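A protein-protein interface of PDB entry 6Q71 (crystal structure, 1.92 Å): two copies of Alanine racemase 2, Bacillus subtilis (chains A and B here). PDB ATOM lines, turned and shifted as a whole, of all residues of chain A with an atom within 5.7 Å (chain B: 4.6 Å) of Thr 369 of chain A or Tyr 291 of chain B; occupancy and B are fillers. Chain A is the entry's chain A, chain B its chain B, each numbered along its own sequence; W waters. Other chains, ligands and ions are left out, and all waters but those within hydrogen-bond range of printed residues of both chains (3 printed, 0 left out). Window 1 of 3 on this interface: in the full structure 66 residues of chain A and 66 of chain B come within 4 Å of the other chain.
Water W3 bridges OE2 of Glu 365 of chain A and OG of Ser 296 of chain B. Water W2 lies within hydrogen-bond range of the side-chain carboxylate (OE2) of Glu 365 of chain A (2.7 Å) and the backbone carbonyl oxygen (O) of Tyr 291 of chain B (2.8 Å). Water W1 bridges the backbone carbonyl oxygen (O) of Ala 292 of chain B (3.0 Å) and the backbone carbonyl oxygen (O) of Ser 368 of chain A (3.4 Å).
Gly 294 of chain A touches none of the printed residues of chain B. Printed residues of chain B within 4 Å of Ile 362 of chain A: Tyr 291 (3.97 Å) and Arg 297 (3.3 Å). Printed residues of chain B within 4 Å of Glu 365 of chain A: Tyr 291 (3.6 Å), Ser 296 (3.9 Å) and Arg 297 (3.1 Å). Of chain B, only Tyr 291 (3.4 Å) comes within 4 Å of Thr 369 of chain A. Printed residues of chain A within 4 Å of Tyr 291 of chain B: Ile 362 (3.97 Å), Tyr 364 (3.0 Å), Glu 365 (3.6 Å), Ser 368 (3.6 Å) and Thr 369 (3.4 Å). Of the printed residues of chain A, Ser 296 of chain B touches Glu 365. Thr 319 of chain B touches none of the printed residues of chain A. The nearest residue of chain B that does not touch Thr 369 of chain A is Ala 292 of chain B (4.5 Å). The nearest printed residue of chain A that does not touch Tyr 291 of chain B is Val 366 of chain A (6.1 Å). The nearest printed residue of chain B that does not touch Ile 362 of chain A is Val 318 of chain B (6.2 Å).
The backbone carbonyl oxygen (O) of Glu 365 of chain A lies within hydrogen-bond range of the side-chain hydroxyl (OG1) of Thr 369 of chain A (2.7 Å). OG1 of Thr 369 of chain A is in hydrogen-bond range of O of Val 366 of chain A, 3.4 Å away. O of Met 320 of chain B lies within hydrogen-bond range of N of Tyr 291 of chain B (3.2 Å). The backbone carbonyl oxygen (O) of Met 320 of chain B sits at hydrogen-bond distance from the backbone NH (N) of Ala 292 of chain B (3.0 Å). OG of Ser 368 of chain A is in hydrogen-bond range of O of Tyr 364 of chain A (2.8 Å). The backbone NH of Tyr 291 of chain B sits at hydrogen-bond distance from the backbone carbonyl oxygen of Thr 319 of chain B (3.0 Å).
Positions printed for both chains: 293 and 294. Of the 10 pairs that touch across the chains among the printed residues, none has its exchanged pair printed and touching as well.
The backbone NH (N) of Arg 297 of chain B lies within hydrogen-bond range of the side-chain carboxylate (OE2) of Glu 365 of chain A (3.1 Å).
Hydrophobic or aromatic side chains of chain A within 4 Å of the printed part of chain B: Ile 362 and Tyr 364. Of the 11 printed residues of chain B, 5 touch a printed residue of chain A. Hydrophobic or aromatic side chains of chain B that line the printed part of chain A: Tyr 291, Ala 292 and Met 320.
Among the printed residues, merely in contact across the chains: Tyr 364 of chain A with Tyr 291 of chain B, Ile 362 of chain A with Arg 297 of chain B, Thr 369 of chain A with Tyr 291 of chain B, Ser 368 of chain A with Tyr 291 of chain B, Glu 365 of chain A with Tyr 291 of chain B, Ser 368 of chain A with Ala 292 of chain B, Tyr 364 of chain A with Met 320 of chain B, Glu 365 of chain A with Ser 296 of chain B and Ile 362 of chain A with Tyr 291 of chain B.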
ATOM      1  N   GLY A  44      24.659 -23.960 -16.336  1.00  0.00           N
ATOM      2  CA  GLY A  44      24.980 -23.174 -15.145  1.00  0.00           C
ATOM      3  C   GLY A  44      24.596 -23.784 -13.798  1.00  0.00           C
ATOM      4  O   GLY A  44      24.791 -23.165 -12.741  1.00  0.00           O
ATOM      5  N   ASP A 293      28.981 -11.571 -11.904  1.00  0.00           N
ATOM      6  CA  ASP A 293      28.378 -12.851 -11.554  1.00  0.00           C
ATOM      7  C   ASP A 293      27.392 -13.362 -12.613  1.00  0.00           C
ATOM      8  O   ASP A 293      26.985 -14.504 -12.549  1.00  0.00           O
ATOM      9  CB  ASP A 293      27.668 -12.744 -10.209  1.00  0.00           C
ATOM     10  CG  ASP A 293      28.595 -12.319  -9.118  1.00  0.00           C
ATOM     11  OD1 ASP A 293      29.471 -13.118  -8.760  1.00  0.00           O
ATOM     12  OD2 ASP A 293      28.516 -11.140  -8.692  1.00  0.00           O
ATOM     13  N   GLY A 294      27.002 -12.503 -13.563  1.00  0.00           N
ATOM     14  CA  GLY A 294      25.997 -12.840 -14.559  1.00  0.00           C
ATOM     15  C   GLY A 294      24.662 -12.166 -14.307  1.00  0.00           C
ATOM     16  O   GLY A 294      23.684 -12.436 -15.023  1.00  0.00           O
ATOM     17  N   ILE A 362      16.131 -15.338 -23.223  1.00  0.00           N
ATOM     18  CA  ILE A 362      15.472 -16.609 -22.912  1.00  0.00           C
ATOM     19  C   ILE A 362      16.073 -17.201 -21.642  1.00  0.00           C
ATOM     20  O   ILE A 362      17.224 -16.912 -21.291  1.00  0.00           O
ATOM     21  CB  ILE A 362      15.618 -17.624 -24.083  1.00  0.00           C
ATOM     22  CG1 ILE A 362      17.086 -17.803 -24.436  1.00  0.00           C
ATOM     23  CG2 ILE A 362      14.820 -17.146 -25.316  1.00  0.00           C
ATOM     24  CD1 ILE A 362      17.366 -18.782 -25.559  1.00  0.00           C
ATOM     25  N   TYR A 364      17.269 -19.976 -20.990  1.00  0.00           N
ATOM     26  CA  TYR A 364      18.552 -20.635 -21.260  1.00  0.00           C
ATOM     27  C   TYR A 364      19.761 -19.711 -20.964  1.00  0.00           C
ATOM     28  O   TYR A 364      20.771 -20.120 -20.349  1.00  0.00           O
ATOM     29  CB  TYR A 364      18.687 -21.066 -22.718  1.00  0.00           C
ATOM     30  CG  TYR A 364      17.760 -22.107 -23.287  1.00  0.00           C
ATOM     31  CD1 TYR A 364      16.434 -21.788 -23.576  1.00  0.00           C
ATOM     32  CD2 TYR A 364      18.239 -23.365 -23.655  1.00  0.00           C
ATOM     33  CE1 TYR A 364      15.598 -22.685 -24.167  1.00  0.00           C
ATOM     34  CE2 TYR A 364      17.377 -24.323 -24.248  1.00  0.00           C
ATOM     35  CZ  TYR A 364      16.054 -23.956 -24.492  1.00  0.00           C
ATOM     36  OH  TYR A 364      15.146 -24.806 -25.079  1.00  0.00           O
ATOM     37  N   GLU A 365      19.677 -18.464 -21.419  1.00  0.00           N
ATOM     38  CA  GLU A 365      20.834 -17.596 -21.284  1.00  0.00           C
ATOM     39  C   GLU A 365      20.996 -17.183 -19.830  1.00  0.00           C
ATOM     40  O   GLU A 365      22.123 -17.116 -19.310  1.00  0.00           O
ATOM     41  CB  GLU A 365      20.736 -16.349 -22.180  1.00  0.00           C
ATOM     42  CG  GLU A 365      22.007 -15.514 -22.145  1.00  0.00           C
ATOM     43  CD  GLU A 365      21.997 -14.308 -23.104  1.00  0.00           C
ATOM     44  OE1 GLU A 365      20.920 -13.759 -23.393  1.00  0.00           O
ATOM     45  OE2 GLU A 365      23.102 -13.938 -23.572  1.00  0.00           O
ATOM     46  N   VAL A 366      19.881 -16.888 -19.181  1.00  0.00           N
ATOM     47  CA  VAL A 366      19.943 -16.392 -17.824  1.00  0.00           C
ATOM     48  C   VAL A 366      20.674 -17.398 -16.909  1.00  0.00           C
ATOM     49  O   VAL A 366      21.529 -16.991 -16.120  1.00  0.00           O
ATOM     50  CB  VAL A 366      18.565 -16.085 -17.266  1.00  0.00           C
ATOM     51  CG1 VAL A 366      18.637 -15.716 -15.785  1.00  0.00           C
ATOM     52  CG2 VAL A 366      17.906 -14.956 -18.096  1.00  0.00           C
ATOM     53  N   VAL A 367      20.357 -18.687 -17.010  1.00  0.00           N
ATOM     54  CA  VAL A 367      20.986 -19.634 -16.091  1.00  0.00           C
ATOM     55  C   VAL A 367      22.394 -20.013 -16.574  1.00  0.00           C
ATOM     56  O   VAL A 367      23.286 -20.130 -15.767  1.00  0.00           O
ATOM     57  CB  VAL A 367      20.104 -20.893 -15.872  1.00  0.00           C
ATOM     58  CG1 VAL A 367      18.811 -20.518 -15.134  1.00  0.00           C
ATOM     59  CG2 VAL A 367      19.803 -21.626 -17.192  1.00  0.00           C
ATOM     60  N   SER A 368      22.614 -20.159 -17.883  1.00  0.00           N
ATOM     61  CA  SER A 368      23.915 -20.659 -18.369  1.00  0.00           C
ATOM     62  C   SER A 368      25.031 -19.615 -18.300  1.00  0.00           C
ATOM     63  O   SER A 368      26.177 -19.963 -18.501  1.00  0.00           O
ATOM     64  CB  SER A 368      23.815 -21.193 -19.794  1.00  0.00           C
ATOM     65  OG  SER A 368      23.519 -20.178 -20.738  1.00  0.00           O
ATOM     66  N   THR A 369      24.691 -18.361 -17.989  1.00  0.00           N
ATOM     67  CA  THR A 369      25.696 -17.317 -17.805  1.00  0.00           C
ATOM     68  C   THR A 369      25.980 -17.017 -16.322  1.00  0.00           C
ATOM     69  O   THR A 369      26.627 -16.032 -16.003  1.00  0.00           O
ATOM     70  CB  THR A 369      25.267 -16.005 -18.490  1.00  0.00           C
ATOM     71  OG1 THR A 369      23.975 -15.621 -17.994  1.00  0.00           O
ATOM     72  CG2 THR A 369      25.221 -16.190 -19.975  1.00  0.00           C
ATOM     73  N   LEU A 370      25.507 -17.859 -15.408  1.00  0.00           N
ATOM     74  CA  LEU A 370      25.862 -17.680 -14.005  1.00  0.00           C
ATOM     75  C   LEU A 370      27.318 -18.091 -13.765  1.00  0.00           C
ATOM     76  O   LEU A 370      27.698 -19.226 -14.014  1.00  0.00           O
ATOM     77  CB  LEU A 370      24.915 -18.484 -13.108  1.00  0.00           C
ATOM     78  CG  LEU A 370      23.515 -17.874 -13.069  1.00  0.00           C
ATOM     79  CD1 LEU A 370      22.440 -18.869 -12.589  1.00  0.00           C
ATOM     80  CD2 LEU A 370      23.529 -16.641 -12.177  1.00  0.00           C
ATOM     81  N   SER A 371      28.110 -17.150 -13.264  1.00  0.00           N
ATOM     82  CA  SER A 371      29.541 -17.292 -13.144  1.00  0.00           C
ATOM     83  C   SER A 371      29.924 -18.432 -12.236  1.00  0.00           C
ATOM     84  O   SER A 371      29.231 -18.737 -11.231  1.00  0.00           O
ATOM     85  CB  SER A 371      30.152 -16.009 -12.590  1.00  0.00           C
ATOM     86  OG  SER A 371      31.490 -16.226 -12.147  1.00  0.00           O
ATOM     87  N   GLY B 290      29.335 -19.192 -28.195  1.00  0.00           N
ATOM     88  CA  GLY B 290      27.919 -18.931 -28.022  1.00  0.00           C
ATOM     89  C   GLY B 290      27.621 -18.131 -26.777  1.00  0.00           C
ATOM     90  O   GLY B 290      28.548 -17.644 -26.113  1.00  0.00           O
ATOM     91  N   TYR B 291      26.348 -17.988 -26.428  1.00  0.00           N
ATOM     92  CA  TYR B 291      26.006 -17.116 -25.312  1.00  0.00           C
ATOM     93  C   TYR B 291      26.424 -17.660 -23.940  1.00  0.00           C
ATOM     94  O   TYR B 291      26.614 -16.852 -23.043  1.00  0.00           O
ATOM     95  CB  TYR B 291      24.506 -16.741 -25.297  1.00  0.00           C
ATOM     96  CG  TYR B 291      23.482 -17.867 -25.266  1.00  0.00           C
ATOM     97  CD1 TYR B 291      23.292 -18.631 -24.116  1.00  0.00           C
ATOM     98  CD2 TYR B 291      22.668 -18.127 -26.363  1.00  0.00           C
ATOM     99  CE1 TYR B 291      22.362 -19.639 -24.052  1.00  0.00           C
ATOM    100  CE2 TYR B 291      21.700 -19.154 -26.307  1.00  0.00           C
ATOM    101  CZ  TYR B 291      21.562 -19.902 -25.137  1.00  0.00           C
ATOM    102  OH  TYR B 291      20.646 -20.953 -25.038  1.00  0.00           O
ATOM    103  N   ALA B 292      26.605 -18.974 -23.764  1.00  0.00           N
ATOM    104  CA  ALA B 292      27.119 -19.464 -22.485  1.00  0.00           C
ATOM    105  C   ALA B 292      28.601 -19.152 -22.317  1.00  0.00           C
ATOM    106  O   ALA B 292      29.138 -19.309 -21.215  1.00  0.00           O
ATOM    107  CB  ALA B 292      26.898 -20.979 -22.324  1.00  0.00           C
ATOM    108  N   ASP B 293      29.265 -18.733 -23.398  1.00  0.00           N
ATOM    109  CA  ASP B 293      30.639 -18.178 -23.303  1.00  0.00           C
ATOM    110  C   ASP B 293      30.680 -16.707 -22.905  1.00  0.00           C
ATOM    111  O   ASP B 293      31.769 -16.171 -22.574  1.00  0.00           O
ATOM    112  CB  ASP B 293      31.385 -18.352 -24.633  1.00  0.00           C
ATOM    113  CG  ASP B 293      31.500 -19.794 -25.033  1.00  0.00           C
ATOM    114  OD1 ASP B 293      32.238 -20.521 -24.341  1.00  0.00           O
ATOM    115  OD2 ASP B 293      30.811 -20.217 -25.986  1.00  0.00           O
ATOM    116  N   GLY B 294      29.511 -16.044 -22.955  1.00  0.00           N
ATOM    117  CA  GLY B 294      29.401 -14.623 -22.680  1.00  0.00           C
ATOM    118  C   GLY B 294      29.231 -13.792 -23.957  1.00  0.00           C
ATOM    119  O   GLY B 294      29.310 -12.552 -23.916  1.00  0.00           O
ATOM    120  N   TYR B 295      29.100 -14.479 -25.091  1.00  0.00           N
ATOM    121  CA  TYR B 295      28.825 -13.822 -26.384  1.00  0.00           C
ATOM    122  C   TYR B 295      27.339 -13.616 -26.489  1.00  0.00           C
ATOM    123  O   TYR B 295      26.590 -14.559 -26.753  1.00  0.00           O
ATOM    124  CB  TYR B 295      29.354 -14.636 -27.571  1.00  0.00           C
ATOM    125  CG  TYR B 295      29.381 -13.846 -28.868  1.00  0.00           C
ATOM    126  CD1 TYR B 295      30.339 -12.874 -29.074  1.00  0.00           C
ATOM    127  CD2 TYR B 295      28.425 -14.060 -29.869  1.00  0.00           C
ATOM    128  CE1 TYR B 295      30.370 -12.122 -30.247  1.00  0.00           C
ATOM    129  CE2 TYR B 295      28.445 -13.334 -31.032  1.00  0.00           C
ATOM    130  CZ  TYR B 295      29.422 -12.355 -31.216  1.00  0.00           C
ATOM    131  OH  TYR B 295      29.465 -11.609 -32.367  1.00  0.00           O
ATOM    132  N   SER B 296      26.929 -12.387 -26.211  1.00  0.00           N
ATOM    133  CA  SER B 296      25.526 -12.057 -25.967  1.00  0.00           C
ATOM    134  C   SER B 296      24.545 -12.520 -27.036  1.00  0.00           C
ATOM    135  O   SER B 296      24.749 -12.305 -28.240  1.00  0.00           O
ATOM    136  CB  SER B 296      25.380 -10.531 -25.806  1.00  0.00           C
ATOM    137  OG  SER B 296      24.023 -10.199 -25.576  1.00  0.00           O
ATOM    138  N   ARG B 297      23.445 -13.115 -26.585  1.00  0.00           N
ATOM    139  CA  ARG B 297      22.376 -13.542 -27.498  1.00  0.00           C
ATOM    140  C   ARG B 297      21.772 -12.328 -28.259  1.00  0.00           C
ATOM    141  O   ARG B 297      21.180 -12.470 -29.332  1.00  0.00           O
ATOM    142  CB  ARG B 297      21.301 -14.305 -26.719  1.00  0.00           C
ATOM    143  CG  ARG B 297      20.279 -15.006 -27.603  1.00  0.00           C
ATOM    144  CD  ARG B 297      19.300 -15.814 -26.787  1.00  0.00           C
ATOM    145  NE  ARG B 297      18.190 -16.329 -27.603  1.00  0.00           N
ATOM    146  CZ  ARG B 297      17.069 -15.656 -27.847  1.00  0.00           C
ATOM    147  NH1 ARG B 297      16.126 -16.205 -28.599  1.00  0.00           N
ATOM    148  NH2 ARG B 297      16.892 -14.427 -27.357  1.00  0.00           N
ATOM    149  N   VAL B 318      22.176 -16.439 -32.115  1.00  0.00           N
ATOM    150  CA  VAL B 318      23.287 -16.974 -31.322  1.00  0.00           C
ATOM    151  C   VAL B 318      22.730 -18.171 -30.541  1.00  0.00           C
ATOM    152  O   VAL B 318      21.611 -18.094 -30.004  1.00  0.00           O
ATOM    153  CB  VAL B 318      23.869 -15.896 -30.380  1.00  0.00           C
ATOM    154  CG1 VAL B 318      24.962 -16.474 -29.419  1.00  0.00           C
ATOM    155  CG2 VAL B 318      24.412 -14.720 -31.206  1.00  0.00           C
ATOM    156  N   THR B 319      23.464 -19.284 -30.514  1.00  0.00           N
ATOM    157  CA  THR B 319      23.008 -20.447 -29.757  1.00  0.00           C
ATOM    158  C   THR B 319      23.904 -20.574 -28.532  1.00  0.00           C
ATOM    159  O   THR B 319      24.816 -19.749 -28.339  1.00  0.00           O
ATOM    160  CB  THR B 319      23.002 -21.762 -30.629  1.00  0.00           C
ATOM    161  OG1 THR B 319      24.330 -22.287 -30.811  1.00  0.00           O
ATOM    162  CG2 THR B 319      22.365 -21.506 -32.001  1.00  0.00           C
ATOM    163  N   MET B 320      23.691 -21.598 -27.719  1.00  0.00           N
ATOM    164  CA  MET B 320      24.350 -21.649 -26.417  1.00  0.00           C
ATOM    165  C   MET B 320      25.876 -21.785 -26.568  1.00  0.00           C
ATOM    166  O   MET B 320      26.625 -21.165 -25.820  1.00  0.00           O
ATOM    167  CB  MET B 320      23.819 -22.783 -25.565  1.00  0.00           C
ATOM    168  CG  MET B 320      24.448 -22.764 -24.159  1.00  0.00           C
ATOM    169  SD  MET B 320      23.783 -24.053 -23.076  1.00  0.00           S
ATOM    170  CE  MET B 320      22.020 -23.567 -23.008  1.00  0.00           C
HETATM  171  O   HOH W   1      28.670 -17.734 -18.713  1.00  0.00           O
HETATM  172  O   HOH W   2      25.804 -14.191 -23.279  1.00  0.00           O
HETATM  173  O   HOH W   3      23.127 -11.487 -22.988  1.00  0.00           O
